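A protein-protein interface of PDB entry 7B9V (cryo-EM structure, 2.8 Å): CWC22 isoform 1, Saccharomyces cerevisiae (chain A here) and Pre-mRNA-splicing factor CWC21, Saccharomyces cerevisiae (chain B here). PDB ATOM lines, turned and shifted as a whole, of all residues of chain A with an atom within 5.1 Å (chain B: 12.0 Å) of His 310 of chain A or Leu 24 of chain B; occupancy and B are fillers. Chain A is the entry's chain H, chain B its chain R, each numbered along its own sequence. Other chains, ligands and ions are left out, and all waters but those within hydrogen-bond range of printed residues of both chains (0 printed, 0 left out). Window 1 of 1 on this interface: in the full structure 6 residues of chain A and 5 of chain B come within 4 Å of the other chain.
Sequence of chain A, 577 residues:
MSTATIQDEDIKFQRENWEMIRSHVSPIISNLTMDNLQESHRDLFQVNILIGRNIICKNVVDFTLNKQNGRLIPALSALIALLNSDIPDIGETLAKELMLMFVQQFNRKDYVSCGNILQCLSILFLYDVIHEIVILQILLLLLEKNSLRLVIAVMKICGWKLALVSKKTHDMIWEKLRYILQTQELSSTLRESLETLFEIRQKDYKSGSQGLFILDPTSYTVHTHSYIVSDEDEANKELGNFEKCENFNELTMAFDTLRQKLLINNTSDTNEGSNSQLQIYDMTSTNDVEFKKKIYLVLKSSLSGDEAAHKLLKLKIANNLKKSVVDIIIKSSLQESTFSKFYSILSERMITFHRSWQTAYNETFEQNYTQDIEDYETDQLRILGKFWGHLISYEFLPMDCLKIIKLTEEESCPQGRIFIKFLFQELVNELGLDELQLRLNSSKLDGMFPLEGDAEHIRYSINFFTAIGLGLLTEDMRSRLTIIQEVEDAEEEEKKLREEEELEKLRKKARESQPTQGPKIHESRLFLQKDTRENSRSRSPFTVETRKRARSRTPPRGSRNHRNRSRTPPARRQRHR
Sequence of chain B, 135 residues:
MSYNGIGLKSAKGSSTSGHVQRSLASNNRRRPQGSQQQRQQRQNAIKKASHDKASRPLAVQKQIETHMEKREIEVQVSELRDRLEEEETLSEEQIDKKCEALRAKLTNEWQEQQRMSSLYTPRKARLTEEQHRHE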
ATOM      1  N   GLY A 305      22.711  18.192 -15.970  1.00  0.00           N
ATOM      2  CA  GLY A 305      23.668  17.396 -15.208  1.00  0.00           C
ATOM      3  C   GLY A 305      23.022  16.372 -14.290  1.00  0.00           C
ATOM      4  O   GLY A 305      23.614  15.323 -14.010  1.00  0.00           O
ATOM      5  N   ASP A 306      21.794  16.653 -13.834  1.00  0.00           N
ATOM      6  CA  ASP A 306      20.961  15.670 -13.136  1.00  0.00           C
ATOM      7  C   ASP A 306      20.598  14.488 -14.028  1.00  0.00           C
ATOM      8  O   ASP A 306      20.664  13.332 -13.591  1.00  0.00           O
ATOM      9  CB  ASP A 306      19.679  16.312 -12.601  1.00  0.00           C
ATOM     10  CG  ASP A 306      19.930  17.555 -11.782  1.00  0.00           C
ATOM     11  OD1 ASP A 306      20.272  18.609 -12.362  1.00  0.00           O
ATOM     12  OD2 ASP A 306      19.744  17.483 -10.549  1.00  0.00           O
ATOM     13  N   GLU A 307      20.197  14.762 -15.273  1.00  0.00           N
ATOM     14  CA  GLU A 307      19.879  13.714 -16.249  1.00  0.00           C
ATOM     15  C   GLU A 307      21.107  12.874 -16.598  1.00  0.00           C
ATOM     16  O   GLU A 307      21.014  11.644 -16.707  1.00  0.00           O
ATOM     17  CB  GLU A 307      19.274  14.318 -17.520  1.00  0.00           C
ATOM     18  CG  GLU A 307      18.688  13.258 -18.461  1.00  0.00           C
ATOM     19  CD  GLU A 307      18.530  13.725 -19.899  1.00  0.00           C
ATOM     20  OE1 GLU A 307      18.672  14.936 -20.162  1.00  0.00           O
ATOM     21  OE2 GLU A 307      18.250  12.870 -20.771  1.00  0.00           O
ATOM     22  N   ALA A 308      22.258  13.526 -16.781  1.00  0.00           N
ATOM     23  CA  ALA A 308      23.526  12.840 -17.047  1.00  0.00           C
ATOM     24  C   ALA A 308      23.926  11.945 -15.884  1.00  0.00           C
ATOM     25  O   ALA A 308      24.364  10.799 -16.089  1.00  0.00           O
ATOM     26  CB  ALA A 308      24.629  13.865 -17.311  1.00  0.00           C
ATOM     27  N   ALA A 309      23.843  12.481 -14.662  1.00  0.00           N
ATOM     28  CA  ALA A 309      24.103  11.696 -13.459  1.00  0.00           C
ATOM     29  C   ALA A 309      23.169  10.509 -13.339  1.00  0.00           C
ATOM     30  O   ALA A 309      23.632   9.415 -13.017  1.00  0.00           O
ATOM     31  CB  ALA A 309      23.970  12.579 -12.232  1.00  0.00           C
ATOM     32  N   HIS A 310      21.865  10.695 -13.598  1.00  0.00           N
ATOM     33  CA  HIS A 310      20.921   9.579 -13.518  1.00  0.00           C
ATOM     34  C   HIS A 310      21.250   8.502 -14.544  1.00  0.00           C
ATOM     35  O   HIS A 310      21.157   7.304 -14.245  1.00  0.00           O
ATOM     36  CB  HIS A 310      19.492  10.081 -13.729  1.00  0.00           C
ATOM     37  CG  HIS A 310      18.521   8.980 -14.022  1.00  0.00           C
ATOM     38  ND1 HIS A 310      18.096   8.076 -13.073  1.00  0.00           N
ATOM     39  CD2 HIS A 310      17.921   8.617 -15.182  1.00  0.00           C
ATOM     40  CE1 HIS A 310      17.265   7.213 -13.632  1.00  0.00           C
ATOM     41  NE2 HIS A 310      17.142   7.519 -14.910  1.00  0.00           N
ATOM     42  N   LYS A 311      21.581   8.915 -15.769  1.00  0.00           N
ATOM     43  CA  LYS A 311      21.877   7.975 -16.846  1.00  0.00           C
ATOM     44  C   LYS A 311      23.137   7.167 -16.552  1.00  0.00           C
ATOM     45  O   LYS A 311      23.207   5.974 -16.869  1.00  0.00           O
ATOM     46  CB  LYS A 311      21.975   8.718 -18.173  1.00  0.00           C
ATOM     47  CG  LYS A 311      20.624   9.062 -18.777  1.00  0.00           C
ATOM     48  CD  LYS A 311      20.751   9.782 -20.100  1.00  0.00           C
ATOM     49  CE  LYS A 311      19.426   9.739 -20.832  1.00  0.00           C
ATOM     50  NZ  LYS A 311      19.353  10.661 -21.993  1.00  0.00           N
ATOM     51  N   LEU A 312      24.146   7.800 -15.934  1.00  0.00           N
ATOM     52  CA  LEU A 312      25.347   7.081 -15.502  1.00  0.00           C
ATOM     53  C   LEU A 312      25.095   6.166 -14.303  1.00  0.00           C
ATOM     54  O   LEU A 312      25.574   5.023 -14.284  1.00  0.00           O
ATOM     55  CB  LEU A 312      26.489   8.054 -15.212  1.00  0.00           C
ATOM     56  CG  LEU A 312      27.176   8.786 -16.352  1.00  0.00           C
ATOM     57  CD1 LEU A 312      28.344   9.581 -15.809  1.00  0.00           C
ATOM     58  CD2 LEU A 312      27.695   7.733 -17.292  1.00  0.00           C
ATOM     59  N   LEU A 313      24.402   6.662 -13.267  1.00  0.00           N
ATOM     60  CA  LEU A 313      24.074   5.841 -12.094  1.00  0.00           C
ATOM     61  C   LEU A 313      23.157   4.657 -12.418  1.00  0.00           C
ATOM     62  O   LEU A 313      23.172   3.655 -11.692  1.00  0.00           O
ATOM     63  CB  LEU A 313      23.474   6.713 -10.985  1.00  0.00           C
ATOM     64  CG  LEU A 313      24.375   7.782 -10.348  1.00  0.00           C
ATOM     65  CD1 LEU A 313      23.587   8.717  -9.444  1.00  0.00           C
ATOM     66  CD2 LEU A 313      25.491   7.139  -9.573  1.00  0.00           C
ATOM     67  N   LYS A 314      22.353   4.744 -13.483  1.00  0.00           N
ATOM     68  CA  LYS A 314      21.509   3.612 -13.863  1.00  0.00           C
ATOM     69  C   LYS A 314      22.328   2.485 -14.499  1.00  0.00           C
ATOM     70  O   LYS A 314      21.894   1.327 -14.479  1.00  0.00           O
ATOM     71  CB  LYS A 314      20.382   4.095 -14.798  1.00  0.00           C
ATOM     72  CG  LYS A 314      19.294   3.074 -15.160  1.00  0.00           C
ATOM     73  CD  LYS A 314      18.528   2.591 -13.931  1.00  0.00           C
ATOM     74  CE  LYS A 314      17.243   1.869 -14.313  1.00  0.00           C
ATOM     75  NZ  LYS A 314      17.526   0.627 -15.085  1.00  0.00           N
ATOM     76  N   PHE A 353      25.870  10.365  -4.171  1.00  0.00           N
ATOM     77  CA  PHE A 353      25.113   9.112  -4.282  1.00  0.00           C
ATOM     78  C   PHE A 353      25.717   7.998  -3.419  1.00  0.00           C
ATOM     79  O   PHE A 353      24.995   7.333  -2.668  1.00  0.00           O
ATOM     80  CB  PHE A 353      25.061   8.669  -5.750  1.00  0.00           C
ATOM     81  CG  PHE A 353      24.253   7.406  -5.993  1.00  0.00           C
ATOM     82  CD1 PHE A 353      22.870   7.472  -6.066  1.00  0.00           C
ATOM     83  CD2 PHE A 353      24.876   6.170  -6.165  1.00  0.00           C
ATOM     84  CE1 PHE A 353      22.117   6.331  -6.303  1.00  0.00           C
ATOM     85  CE2 PHE A 353      24.122   5.024  -6.403  1.00  0.00           C
ATOM     86  CZ  PHE A 353      22.742   5.112  -6.470  1.00  0.00           C
ATOM     87  N   ILE B   6       2.919  11.417 -10.106  1.00  0.00           N
ATOM     88  CA  ILE B   6       3.893  11.684 -11.158  1.00  0.00           C
ATOM     89  C   ILE B   6       3.349  11.087 -12.455  1.00  0.00           C
ATOM     90  O   ILE B   6       2.677  10.049 -12.451  1.00  0.00           O
ATOM     91  CB  ILE B   6       5.272  11.053 -10.826  1.00  0.00           C
ATOM     92  CG1 ILE B   6       5.696  11.329  -9.384  1.00  0.00           C
ATOM     93  CG2 ILE B   6       6.377  11.601 -11.728  1.00  0.00           C
ATOM     94  CD1 ILE B   6       5.917  12.759  -9.066  1.00  0.00           C
ATOM     95  N   HIS B  19       6.734   6.652 -20.196  1.00  0.00           N
ATOM     96  CA  HIS B  19       7.507   5.907 -19.216  1.00  0.00           C
ATOM     97  C   HIS B  19       8.101   6.876 -18.205  1.00  0.00           C
ATOM     98  O   HIS B  19       8.657   7.913 -18.582  1.00  0.00           O
ATOM     99  CB  HIS B  19       8.604   5.110 -19.913  1.00  0.00           C
ATOM    100  CG  HIS B  19       9.405   4.256 -18.985  1.00  0.00           C
ATOM    101  ND1 HIS B  19      10.733   4.500 -18.709  1.00  0.00           N
ATOM    102  CD2 HIS B  19       9.065   3.163 -18.267  1.00  0.00           C
ATOM    103  CE1 HIS B  19      11.175   3.593 -17.858  1.00  0.00           C
ATOM    104  NE2 HIS B  19      10.182   2.769 -17.574  1.00  0.00           N
ATOM    105  N   VAL B  20       7.991   6.531 -16.923  1.00  0.00           N
ATOM    106  CA  VAL B  20       8.500   7.333 -15.820  1.00  0.00           C
ATOM    107  C   VAL B  20       9.497   6.483 -15.036  1.00  0.00           C
ATOM    108  O   VAL B  20       9.297   5.276 -14.864  1.00  0.00           O
ATOM    109  CB  VAL B  20       7.335   7.843 -14.925  1.00  0.00           C
ATOM    110  CG1 VAL B  20       7.806   8.736 -13.780  1.00  0.00           C
ATOM    111  CG2 VAL B  20       6.310   8.620 -15.755  1.00  0.00           C
ATOM    112  N   GLN B  21      10.579   7.112 -14.579  1.00  0.00           N
ATOM    113  CA  GLN B  21      11.604   6.458 -13.786  1.00  0.00           C
ATOM    114  C   GLN B  21      12.135   7.463 -12.770  1.00  0.00           C
ATOM    115  O   GLN B  21      12.268   8.654 -13.071  1.00  0.00           O
ATOM    116  CB  GLN B  21      12.728   5.897 -14.676  1.00  0.00           C
ATOM    117  CG  GLN B  21      13.439   6.929 -15.540  1.00  0.00           C
ATOM    118  CD  GLN B  21      14.171   6.332 -16.721  1.00  0.00           C
ATOM    119  OE1 GLN B  21      15.328   5.925 -16.608  1.00  0.00           O
ATOM    120  NE2 GLN B  21      13.503   6.274 -17.866  1.00  0.00           N
ATOM    121  N   ARG B  22      12.296   7.000 -11.529  1.00  0.00           N
ATOM    122  CA  ARG B  22      12.787   7.853 -10.456  1.00  0.00           C
ATOM    123  C   ARG B  22      14.238   8.259 -10.702  1.00  0.00           C
ATOM    124  O   ARG B  22      15.042   7.483 -11.229  1.00  0.00           O
ATOM    125  CB  ARG B  22      12.638   7.172  -9.089  1.00  0.00           C
ATOM    126  CG  ARG B  22      13.438   5.890  -8.858  1.00  0.00           C
ATOM    127  CD  ARG B  22      13.613   5.627  -7.373  1.00  0.00           C
ATOM    128  NE  ARG B  22      14.450   6.657  -6.756  1.00  0.00           N
ATOM    129  CZ  ARG B  22      15.602   6.424  -6.145  1.00  0.00           C
ATOM    130  NH1 ARG B  22      16.107   5.198  -6.060  1.00  0.00           N
ATOM    131  NH2 ARG B  22      16.273   7.445  -5.616  1.00  0.00           N
ATOM    132  N   SER B  23      14.558   9.501 -10.350  1.00  0.00           N
ATOM    133  CA  SER B  23      15.900  10.040 -10.545  1.00  0.00           C
ATOM    134  C   SER B  23      16.823   9.506  -9.458  1.00  0.00           C
ATOM    135  O   SER B  23      16.649   9.819  -8.276  1.00  0.00           O
ATOM    136  CB  SER B  23      15.872  11.566 -10.527  1.00  0.00           C
ATOM    137  OG  SER B  23      17.168  12.108 -10.719  1.00  0.00           O
ATOM    138  N   LEU B  24      17.809   8.696  -9.862  1.00  0.00           N
ATOM    139  CA  LEU B  24      18.857   8.237  -8.954  1.00  0.00           C
ATOM    140  C   LEU B  24      19.745   9.377  -8.461  1.00  0.00           C
ATOM    141  O   LEU B  24      20.375   9.245  -7.404  1.00  0.00           O
ATOM    142  CB  LEU B  24      19.708   7.182  -9.661  1.00  0.00           C
ATOM    143  CG  LEU B  24      19.014   5.845  -9.914  1.00  0.00           C
ATOM    144  CD1 LEU B  24      19.860   4.973 -10.806  1.00  0.00           C
ATOM    145  CD2 LEU B  24      18.743   5.127  -8.612  1.00  0.00           C
ATOM    146  N   ALA B  25      19.799  10.491  -9.200  1.00  0.00           N
ATOM    147  CA  ALA B  25      20.519  11.685  -8.776  1.00  0.00           C
ATOM    148  C   ALA B  25      19.843  12.394  -7.607  1.00  0.00           C
ATOM    149  O   ALA B  25      20.502  13.178  -6.917  1.00  0.00           O
ATOM    150  CB  ALA B  25      20.665  12.660  -9.945  1.00  0.00           C
ATOM    151  N   SER B  26      18.553  12.157  -7.381  1.00  0.00           N
ATOM    152  CA  SER B  26      17.833  12.772  -6.268  1.00  0.00           C
ATOM    153  C   SER B  26      17.999  11.986  -4.970  1.00  0.00           C
ATOM    154  O   SER B  26      18.867  12.303  -4.155  1.00  0.00           O
ATOM    155  CB  SER B  26      16.343  12.897  -6.604  1.00  0.00           C
ATOM    156  OG  SER B  26      15.624  13.523  -5.555  1.00  0.00           O
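OE1 of Gln 21 of chain B lies within hydrogen-bond range of NE2 of His 310 of chain A (3.0 Å).
A ring nitrogen (ND1) of His 310 of chain A lies within hydrogen-bond range of the backbone NH (N) of Leu 24 of chain B (3.3 Å).
A ring nitrogen (ND1) of His 19 of chain B sits at hydrogen-bond distance from the side-chain amide nitrogen of Gln 21 of chain B (3.4 Å).
OG of Ser 23 of chain B lies close to N of Ala 25 of chain B (3.4 Å).
Among the printed residues, merely in contact across the chains: Asp 306 of chain A with Ala 25 of chain B (3.7 Å), His 310 of chain A with Arg 22 of chain B (3.3 Å), His 310 of chain A with Ser 23 of chain B (3.9 Å), Leu 313 of chain A with Leu 24 of chain B (3.7 Å), Lys 314 of chain A with Leu 24 of chain B (3.7 Å) and Phe 353 of chain A with Leu 24 of chain B (3.3 Å).
No residue of chain B comes within 4 Å of Gly 305 of chain A.
Of the printed residues of chain B, Asp 306 of chain A touches Ala 25 (3.7 Å).
Of the printed residues of chain B, His 310 of chain A touches Gln 21 (3.0 Å), Arg 22 (3.3 Å), Ser 23 (3.9 Å) and Leu 24 (3.3 Å).
No residue of chain B comes within 4 Å of Lys 311 of chain A.
Leu 313 of chain A touches just one residue of chain B: Leu 24 (3.7 Å).
Of chain B, only Leu 24 comes within 4 Å of Lys 314 of chain A.
Of chain B, only Leu 24 (3.3 Å) comes within 4 Å of Phe 353 of chain A.
Ile 6 of chain B touches none of the printed residues of chain A.
Printed residues of chain A within 4 Å of Gln 21 of chain B: His 310 (3.0 Å).
Of the printed residues of chain A, Arg 22 of chain B touches His 310.
Of the printed residues of chain A, Ser 23 of chain B touches His 310 (3.9 Å).
Of chain A, only His 310, Leu 313, Lys 314 and Phe 353 come within 4 Å of Leu 24 of chain B.
Printed residues of chain A within 4 Å of Ala 25 of chain B: Asp 306.
Ser 26 of chain B touches none of the printed residues of chain A.
The nearest printed residue of chain A that does not touch Leu 24 of chain B is Ala 309 of chain A (5.6 Å).
The nearest printed residue of chain B that does not touch Asp 306 of chain A is Ser 23 of chain B (4.7 Å).
Printed residues of chain A that touch a printed residue of chain B: Asp 306, His 310, Leu 313, Lys 314 and Phe 353.
Hydrophobic or aromatic side chains of chain A that line the printed part of chain B: His 310, Leu 313 and Phe 353.
Along chain A the printed residues that touch a printed residue of chain B span positions 306 to 353.
Among the printed residues, no Asp or Glu carboxylate lies within 4 Å of a Lys or Arg side-chain nitrogen of the other chain.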
